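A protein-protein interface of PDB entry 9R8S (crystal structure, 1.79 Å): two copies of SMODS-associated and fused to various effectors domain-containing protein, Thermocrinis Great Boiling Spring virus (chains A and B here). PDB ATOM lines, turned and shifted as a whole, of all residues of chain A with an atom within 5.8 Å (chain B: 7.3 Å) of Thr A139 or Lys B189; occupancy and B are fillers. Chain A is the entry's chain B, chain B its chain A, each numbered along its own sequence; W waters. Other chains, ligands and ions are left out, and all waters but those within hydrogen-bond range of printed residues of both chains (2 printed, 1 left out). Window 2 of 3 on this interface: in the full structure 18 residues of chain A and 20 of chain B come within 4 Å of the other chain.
The side-chain carboxylate (OE1) of Glu A136 is in salt-bridge range of the guanidinium group (NH2) of Arg B108, 3.0 Å away.
NZ of Lys B124 is in salt-bridge range of OE1 of Glu A143, 3.3 Å away.
The side-chain amide oxygen (OE1) of Gln B185 lies within hydrogen-bond range of the backbone NH (N) of Glu A136, at 3.2 Å.
O of Lys B188 sits at hydrogen-bond distance from OG1 of Thr A139 (2.5 Å).
O of Gln B191 lies within hydrogen-bond range of OG1 of Thr A139, 3.5 Å away.
Of the 9 printed residues of chain A, 4 touch a printed residue of chain B.
Printed residues of chain B that touch a printed residue of chain A: Arg B108, Lys B124, Gln B185, Lys B188, Lys B189, Gln B191 and Ser B192.
Among the printed residues, Asp or Glu carboxylates within 4 Å of a Lys or Arg side-chain nitrogen of the other chain: Glu A136 with Arg B108 (3.0 Å) and Glu A143 with Lys B124 (3.3 Å).
Printed residues of chain B within 4 Å of Glu A136: Arg B108 (3.0 Å), Gln B185 (3.2 Å), Lys B188 (3.8 Å) and Lys B189 (3.6 Å).
Thr A139 touches four residues of chain B.
Of the printed residues of chain B, Ala A140 touches Ser B192.
Printed residues of chain A within 4 Å of Arg B108: Glu A136.
Leu B184 touches none of the printed residues of chain A.
Of the printed residues of chain A, Gln B185 touches Glu A136.
Val B187 touches none of the printed residues of chain A.
Of the printed residues of chain A, Lys B188 touches Glu A136 (3.8 Å) and Thr A139 (2.5 Å).
Of chain A, only Glu A136 (3.6 Å) and Thr A139 (3.6 Å) come within 4 Å of Lys B189.
The nearest printed residue of chain A that does not touch Lys B189 is Lys A138 (6.1 Å).
The nearest printed residue of chain A that does not touch Arg B108 is Ile A137 (6.0 Å).
The guanidinium group (NH2) of Arg B108 lies within salt-bridge range of the side-chain carboxylate (OD1) of Asp B186, at 3.0 Å.
OE1 of Gln B191 sits at hydrogen-bond distance from NZ of Lys B124 (3.3 Å).
The backbone carbonyl oxygen of Ser B192 is in hydrogen-bond range of the side-chain amino group of Lys B124 (3.0 Å).
OE1 of Gln B185 lies within hydrogen-bond range of NZ of Lys B188 (2.9 Å).
OE2 of Glu A136 lies within hydrogen-bond range of N of Lys A138, at 3.2 Å.
No position is printed for both chains.
Of the 11 pairs that touch across the chains among the printed residues, none has its exchanged pair printed and touching as well.
Water W2 lies within hydrogen-bond range of the backbone NH (N) of Thr A139 (2.8 Å), the side-chain carboxylate (OE2) of Glu A136 (2.9 Å), the backbone carbonyl oxygen (O) of Lys B188 (3.0 Å) and the backbone NH (N) of Lys A138 (3.3 Å).
Water W1 lies within hydrogen-bond range of OG of Ser B192 (3.0 Å), OE2 of Glu A143 (3.1 Å) and O of Phe B193 (3.3 Å).
Among the printed residues, merely in contact across the chains: Glu A136 with Lys B188 (3.8 Å), Glu A136 with Lys B189 (3.6 Å), Thr A139 with Lys B189 (3.6 Å), Thr A139 with Ser B192 (3.5 Å), Ala A140 with Ser B192 (3.6 Å) and Glu A143 with Ser B192 (3.7 Å).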
ATOM      1  N   GLU A 136      -5.785  10.943  30.459  1.00  0.00           N
ATOM      2  CA  GLU A 136      -4.424  11.405  30.230  1.00  0.00           C
ATOM      3  C   GLU A 136      -4.444  12.566  29.236  1.00  0.00           C
ATOM      4  O   GLU A 136      -4.988  12.395  28.155  1.00  0.00           O
ATOM      5  CB  GLU A 136      -3.645  10.214  29.670  1.00  0.00           C
ATOM      6  CG  GLU A 136      -2.249  10.556  29.171  1.00  0.00           C
ATOM      7  CD  GLU A 136      -1.382  11.205  30.227  1.00  0.00           C
ATOM      8  OE1 GLU A 136      -1.318  10.667  31.352  1.00  0.00           O
ATOM      9  OE2 GLU A 136      -0.749  12.224  29.907  1.00  0.00           O
ATOM     10  N   ILE A 137      -3.859  13.724  29.594  1.00  0.00           N
ATOM     11  CA  ILE A 137      -4.064  14.932  28.804  1.00  0.00           C
ATOM     12  C   ILE A 137      -2.774  15.524  28.245  1.00  0.00           C
ATOM     13  O   ILE A 137      -2.886  16.475  27.483  1.00  0.00           O
ATOM     14  CB  ILE A 137      -4.815  16.017  29.597  1.00  0.00           C
ATOM     15  CG1 ILE A 137      -4.002  16.532  30.790  1.00  0.00           C
ATOM     16  CG2 ILE A 137      -6.206  15.524  29.986  1.00  0.00           C
ATOM     17  CD1 ILE A 137      -4.536  17.817  31.402  1.00  0.00           C
ATOM     18  N   LYS A 138      -1.581  15.010  28.582  1.00  0.00           N
ATOM     19  CA  LYS A 138      -0.351  15.729  28.257  1.00  0.00           C
ATOM     20  C   LYS A 138      -0.222  15.962  26.747  1.00  0.00           C
ATOM     21  O   LYS A 138       0.032  17.094  26.322  1.00  0.00           O
ATOM     22  CB  LYS A 138       0.902  15.027  28.778  1.00  0.00           C
ATOM     23  CG  LYS A 138       2.251  15.677  28.465  1.00  0.00           C
ATOM     24  CD  LYS A 138       3.449  14.838  28.921  1.00  0.00           C
ATOM     25  CE  LYS A 138       4.807  15.524  28.862  1.00  0.00           C
ATOM     26  NZ  LYS A 138       5.135  16.393  30.007  1.00  0.00           N
ATOM     27  N   THR A 139      -0.361  14.902  25.937  1.00  0.00           N
ATOM     28  CA  THR A 139      -0.165  15.056  24.504  1.00  0.00           C
ATOM     29  C   THR A 139      -1.272  15.926  23.913  1.00  0.00           C
ATOM     30  O   THR A 139      -1.004  16.687  22.980  1.00  0.00           O
ATOM     31  CB  THR A 139      -0.038  13.720  23.770  1.00  0.00           C
ATOM     32  OG1 THR A 139      -1.167  12.905  24.089  1.00  0.00           O
ATOM     33  CG2 THR A 139       1.285  13.054  24.105  1.00  0.00           C
ATOM     34  N   ALA A 140      -2.501  15.831  24.434  1.00  0.00           N
ATOM     35  CA  ALA A 140      -3.592  16.656  23.914  1.00  0.00           C
ATOM     36  C   ALA A 140      -3.318  18.145  24.158  1.00  0.00           C
ATOM     37  O   ALA A 140      -3.582  18.960  23.271  1.00  0.00           O
ATOM     38  CB  ALA A 140      -4.934  16.245  24.493  1.00  0.00           C
ATOM     39  N   VAL A 141      -2.791  18.487  25.343  1.00  0.00           N
ATOM     40  CA  VAL A 141      -2.520  19.880  25.667  1.00  0.00           C
ATOM     41  C   VAL A 141      -1.389  20.387  24.773  1.00  0.00           C
ATOM     42  O   VAL A 141      -1.502  21.466  24.198  1.00  0.00           O
ATOM     43  CB  VAL A 141      -2.205  20.102  27.155  1.00  0.00           C
ATOM     44  CG1 VAL A 141      -1.648  21.509  27.437  1.00  0.00           C
ATOM     45  CG2 VAL A 141      -3.426  19.814  28.016  1.00  0.00           C
ATOM     46  N   LYS A 142      -0.310  19.604  24.632  1.00  0.00           N
ATOM     47  CA  LYS A 142       0.827  20.062  23.841  1.00  0.00           C
ATOM     48  C   LYS A 142       0.436  20.293  22.375  1.00  0.00           C
ATOM     49  O   LYS A 142       0.874  21.264  21.762  1.00  0.00           O
ATOM     50  CB  LYS A 142       2.023  19.114  23.937  1.00  0.00           C
ATOM     51  CG  LYS A 142       2.675  19.120  25.310  1.00  0.00           C
ATOM     52  CD  LYS A 142       4.096  18.588  25.320  1.00  0.00           C
ATOM     53  CE  LYS A 142       4.809  19.021  26.558  1.00  0.00           C
ATOM     54  NZ  LYS A 142       6.150  18.442  26.630  1.00  0.00           N
ATOM     55  N   GLU A 143      -0.391  19.405  21.824  1.00  0.00           N
ATOM     56  CA  GLU A 143      -0.828  19.528  20.445  1.00  0.00           C
ATOM     57  C   GLU A 143      -1.622  20.820  20.268  1.00  0.00           C
ATOM     58  O   GLU A 143      -1.425  21.548  19.294  1.00  0.00           O
ATOM     59  CB  GLU A 143      -1.658  18.306  20.061  1.00  0.00           C
ATOM     60  CG  GLU A 143      -2.134  18.323  18.613  1.00  0.00           C
ATOM     61  CD  GLU A 143      -2.587  16.950  18.149  1.00  0.00           C
ATOM     62  OE1 GLU A 143      -1.698  16.083  17.986  1.00  0.00           O
ATOM     63  OE2 GLU A 143      -3.814  16.743  18.000  1.00  0.00           O
ATOM     64  N   TYR A 144      -2.524  21.086  21.216  1.00  0.00           N
ATOM     65  CA  TYR A 144      -3.319  22.305  21.202  1.00  0.00           C
ATOM     66  C   TYR A 144      -2.419  23.536  21.305  1.00  0.00           C
ATOM     67  O   TYR A 144      -2.590  24.499  20.565  1.00  0.00           O
ATOM     68  CB  TYR A 144      -4.322  22.316  22.352  1.00  0.00           C
ATOM     69  CG  TYR A 144      -5.025  23.654  22.525  1.00  0.00           C
ATOM     70  CD1 TYR A 144      -6.018  24.069  21.639  1.00  0.00           C
ATOM     71  CD2 TYR A 144      -4.696  24.501  23.576  1.00  0.00           C
ATOM     72  CE1 TYR A 144      -6.672  25.281  21.811  1.00  0.00           C
ATOM     73  CE2 TYR A 144      -5.335  25.718  23.745  1.00  0.00           C
ATOM     74  CZ  TYR A 144      -6.324  26.110  22.859  1.00  0.00           C
ATOM     75  OH  TYR A 144      -6.945  27.322  23.030  1.00  0.00           O
ATOM     76  N   ARG B 108      -4.919   4.984  37.968  1.00  0.00           N
ATOM     77  CA  ARG B 108      -3.888   4.838  36.947  1.00  0.00           C
ATOM     78  C   ARG B 108      -2.668   4.166  37.575  1.00  0.00           C
ATOM     79  O   ARG B 108      -2.324   4.486  38.700  1.00  0.00           O
ATOM     80  CB  ARG B 108      -3.536   6.191  36.331  1.00  0.00           C
ATOM     81  CG  ARG B 108      -4.663   6.800  35.505  1.00  0.00           C
ATOM     82  CD  ARG B 108      -4.713   6.253  34.086  1.00  0.00           C
ATOM     83  NE  ARG B 108      -3.494   6.523  33.318  1.00  0.00           N
ATOM     84  CZ  ARG B 108      -3.107   7.737  32.911  1.00  0.00           C
ATOM     85  NH1 ARG B 108      -3.917   8.780  33.051  1.00  0.00           N
ATOM     86  NH2 ARG B 108      -1.933   7.887  32.321  1.00  0.00           N
ATOM     87  N   LEU B 109      -2.043   3.224  36.852  1.00  0.00           N
ATOM     88  CA  LEU B 109      -1.064   2.315  37.440  1.00  0.00           C
ATOM     89  C   LEU B 109       0.313   2.514  36.822  1.00  0.00           C
ATOM     90  O   LEU B 109       0.418   2.916  35.670  1.00  0.00           O
ATOM     91  CB  LEU B 109      -1.512   0.870  37.220  1.00  0.00           C
ATOM     92  CG  LEU B 109      -2.881   0.498  37.793  1.00  0.00           C
ATOM     93  CD1 LEU B 109      -3.229  -0.878  37.268  1.00  0.00           C
ATOM     94  CD2 LEU B 109      -2.931   0.538  39.318  1.00  0.00           C
ATOM     95  N   LYS B 110       1.353   2.219  37.619  1.00  0.00           N
ATOM     96  CA  LYS B 110       2.711   2.084  37.122  1.00  0.00           C
ATOM     97  C   LYS B 110       3.052   0.608  36.961  1.00  0.00           C
ATOM     98  O   LYS B 110       3.865   0.262  36.120  1.00  0.00           O
ATOM     99  CB  LYS B 110       3.753   2.708  38.062  1.00  0.00           C
ATOM    100  CG  LYS B 110       3.593   4.201  38.273  1.00  0.00           C
ATOM    101  CD  LYS B 110       3.719   5.075  37.032  1.00  0.00           C
ATOM    102  CE  LYS B 110       3.396   6.506  37.353  1.00  0.00           C
ATOM    103  NZ  LYS B 110       3.844   7.349  36.251  1.00  0.00           N
ATOM    104  N   LYS B 124      -3.202   8.935  13.741  1.00  0.00           N
ATOM    105  CA  LYS B 124      -4.007   9.437  14.843  1.00  0.00           C
ATOM    106  C   LYS B 124      -5.297   8.639  15.035  1.00  0.00           C
ATOM    107  O   LYS B 124      -6.016   8.895  15.995  1.00  0.00           O
ATOM    108  CB  LYS B 124      -4.279  10.933  14.635  1.00  0.00           C
ATOM    109  CG  LYS B 124      -3.025  11.773  14.772  1.00  0.00           C
ATOM    110  CD  LYS B 124      -3.236  13.148  15.389  1.00  0.00           C
ATOM    111  CE  LYS B 124      -1.932  13.826  15.697  1.00  0.00           C
ATOM    112  NZ  LYS B 124      -1.077  13.115  16.664  1.00  0.00           N
ATOM    113  N   LEU B 184      -5.235   2.072  28.403  1.00  0.00           N
ATOM    114  CA  LEU B 184      -5.923   2.827  27.360  1.00  0.00           C
ATOM    115  C   LEU B 184      -5.668   4.330  27.510  1.00  0.00           C
ATOM    116  O   LEU B 184      -5.749   5.071  26.524  1.00  0.00           O
ATOM    117  CB  LEU B 184      -7.422   2.534  27.362  1.00  0.00           C
ATOM    118  CG  LEU B 184      -7.825   1.154  26.838  1.00  0.00           C
ATOM    119  CD1 LEU B 184      -9.287   0.885  27.101  1.00  0.00           C
ATOM    120  CD2 LEU B 184      -7.518   1.062  25.359  1.00  0.00           C
ATOM    121  N   GLN B 185      -5.378   4.784  28.732  1.00  0.00           N
ATOM    122  CA  GLN B 185      -4.980   6.169  28.950  1.00  0.00           C
ATOM    123  C   GLN B 185      -3.473   6.303  28.735  1.00  0.00           C
ATOM    124  O   GLN B 185      -3.027   7.275  28.160  1.00  0.00           O
ATOM    125  CB  GLN B 185      -5.457   6.646  30.326  1.00  0.00           C
ATOM    126  CG  GLN B 185      -6.975   6.612  30.504  1.00  0.00           C
ATOM    127  CD  GLN B 185      -7.718   7.416  29.452  1.00  0.00           C
ATOM    128  OE1 GLN B 185      -7.312   8.528  29.087  1.00  0.00           O
ATOM    129  NE2 GLN B 185      -8.808   6.865  28.942  1.00  0.00           N
ATOM    130  N   ASP B 186      -2.681   5.328  29.189  1.00  0.00           N
ATOM    131  CA  ASP B 186      -1.231   5.372  29.048  1.00  0.00           C
ATOM    132  C   ASP B 186      -0.791   5.488  27.590  1.00  0.00           C
ATOM    133  O   ASP B 186       0.215   6.124  27.320  1.00  0.00           O
ATOM    134  CB  ASP B 186      -0.529   4.164  29.673  1.00  0.00           C
ATOM    135  CG  ASP B 186      -0.363   4.180  31.193  1.00  0.00           C
ATOM    136  OD1 ASP B 186      -0.814   5.162  31.846  1.00  0.00           O
ATOM    137  OD2 ASP B 186       0.231   3.200  31.735  1.00  0.00           O
ATOM    138  N   VAL B 187      -1.492   4.845  26.652  1.00  0.00           N
ATOM    139  CA  VAL B 187      -1.092   4.876  25.251  1.00  0.00           C
ATOM    140  C   VAL B 187      -1.096   6.309  24.709  1.00  0.00           C
ATOM    141  O   VAL B 187      -0.375   6.606  23.761  1.00  0.00           O
ATOM    142  CB  VAL B 187      -1.998   3.960  24.401  1.00  0.00           C
ATOM    143  CG1 VAL B 187      -3.407   4.521  24.239  1.00  0.00           C
ATOM    144  CG2 VAL B 187      -1.402   3.655  23.035  1.00  0.00           C
ATOM    145  N   LYS B 188      -1.883   7.203  25.315  1.00  0.00           N
ATOM    146  CA  LYS B 188      -1.969   8.593  24.864  1.00  0.00           C
ATOM    147  C   LYS B 188      -0.693   9.386  25.160  1.00  0.00           C
ATOM    148  O   LYS B 188      -0.541  10.506  24.676  1.00  0.00           O
ATOM    149  CB  LYS B 188      -3.151   9.288  25.542  1.00  0.00           C
ATOM    150  CG  LYS B 188      -4.523   8.737  25.166  1.00  0.00           C
ATOM    151  CD  LYS B 188      -5.634   9.439  25.930  1.00  0.00           C
ATOM    152  CE  LYS B 188      -6.974   8.849  25.686  1.00  0.00           C
ATOM    153  NZ  LYS B 188      -7.996   9.527  26.480  1.00  0.00           N
ATOM    154  N   LYS B 189       0.226   8.820  25.950  1.00  0.00           N
ATOM    155  CA  LYS B 189       1.546   9.398  26.150  1.00  0.00           C
ATOM    156  C   LYS B 189       2.373   9.320  24.871  1.00  0.00           C
ATOM    157  O   LYS B 189       3.257  10.141  24.670  1.00  0.00           O
ATOM    158  CB  LYS B 189       2.306   8.712  27.290  1.00  0.00           C
ATOM    159  CG  LYS B 189       1.692   8.942  28.665  1.00  0.00           C
ATOM    160  CD  LYS B 189       2.403   8.277  29.838  1.00  0.00           C
ATOM    161  CE  LYS B 189       1.657   8.617  31.089  1.00  0.00           C
ATOM    162  NZ  LYS B 189       2.148   7.957  32.297  1.00  0.00           N
ATOM    163  N   HIS B 190       2.094   8.343  24.006  1.00  0.00           N
ATOM    164  CA  HIS B 190       2.817   8.217  22.744  1.00  0.00           C
ATOM    165  C   HIS B 190       2.510   9.412  21.841  1.00  0.00           C
ATOM    166  O   HIS B 190       3.405   9.998  21.260  1.00  0.00           O
ATOM    167  CB  HIS B 190       2.484   6.908  22.017  1.00  0.00           C
ATOM    168  CG  HIS B 190       2.937   5.654  22.709  1.00  0.00           C
ATOM    169  ND1 HIS B 190       4.263   5.360  22.933  1.00  0.00           N
ATOM    170  CD2 HIS B 190       2.239   4.614  23.199  1.00  0.00           C
ATOM    171  CE1 HIS B 190       4.353   4.190  23.562  1.00  0.00           C
ATOM    172  NE2 HIS B 190       3.137   3.721  23.729  1.00  0.00           N
ATOM    173  N   GLN B 191       1.229   9.742  21.692  1.00  0.00           N
ATOM    174  CA  GLN B 191       0.786  10.836  20.839  1.00  0.00           C
ATOM    175  C   GLN B 191      -0.681  11.114  21.155  1.00  0.00           C
ATOM    176  O   GLN B 191      -1.325  10.307  21.822  1.00  0.00           O
ATOM    177  CB  GLN B 191       0.975  10.532  19.346  1.00  0.00           C
ATOM    178  CG  GLN B 191       0.172   9.337  18.834  1.00  0.00           C
ATOM    179  CD  GLN B 191       0.286   9.124  17.336  1.00  0.00           C
ATOM    180  OE1 GLN B 191       0.117  10.035  16.523  1.00  0.00           O
ATOM    181  NE2 GLN B 191       0.571   7.899  16.935  1.00  0.00           N
ATOM    182  N   SER B 192      -1.198  12.244  20.651  1.00  0.00           N
ATOM    183  CA  SER B 192      -2.604  12.580  20.821  1.00  0.00           C
ATOM    184  C   SER B 192      -3.403  11.965  19.678  1.00  0.00           C
ATOM    185  O   SER B 192      -3.292  12.401  18.539  1.00  0.00           O
ATOM    186  CB  SER B 192      -2.828  14.074  20.892  1.00  0.00           C
ATOM    187  OG  SER B 192      -4.178  14.363  21.255  1.00  0.00           O
ATOM    188  N   PHE B 193      -4.210  10.958  19.990  1.00  0.00           N
ATOM    189  CA  PHE B 193      -5.020  10.275  18.997  1.00  0.00           C
ATOM    190  C   PHE B 193      -6.314  11.047  18.784  1.00  0.00           C
ATOM    191  O   PHE B 193      -6.812  11.666  19.705  1.00  0.00           O
ATOM    192  CB  PHE B 193      -5.324   8.854  19.480  1.00  0.00           C
ATOM    193  CG  PHE B 193      -4.066   8.014  19.635  1.00  0.00           C
ATOM    194  CD1 PHE B 193      -3.462   7.449  18.519  1.00  0.00           C
ATOM    195  CD2 PHE B 193      -3.491   7.808  20.885  1.00  0.00           C
ATOM    196  CE1 PHE B 193      -2.298   6.716  18.651  1.00  0.00           C
ATOM    197  CE2 PHE B 193      -2.331   7.057  21.005  1.00  0.00           C
ATOM    198  CZ  PHE B 193      -1.745   6.506  19.893  1.00  0.00           C
HETATM  199  O   HOH W   1      -6.035  14.750  18.992  1.00  0.00           O
HETATM  200  O   HOH W   2      -0.448  12.343  27.029  1.00  0.00           O
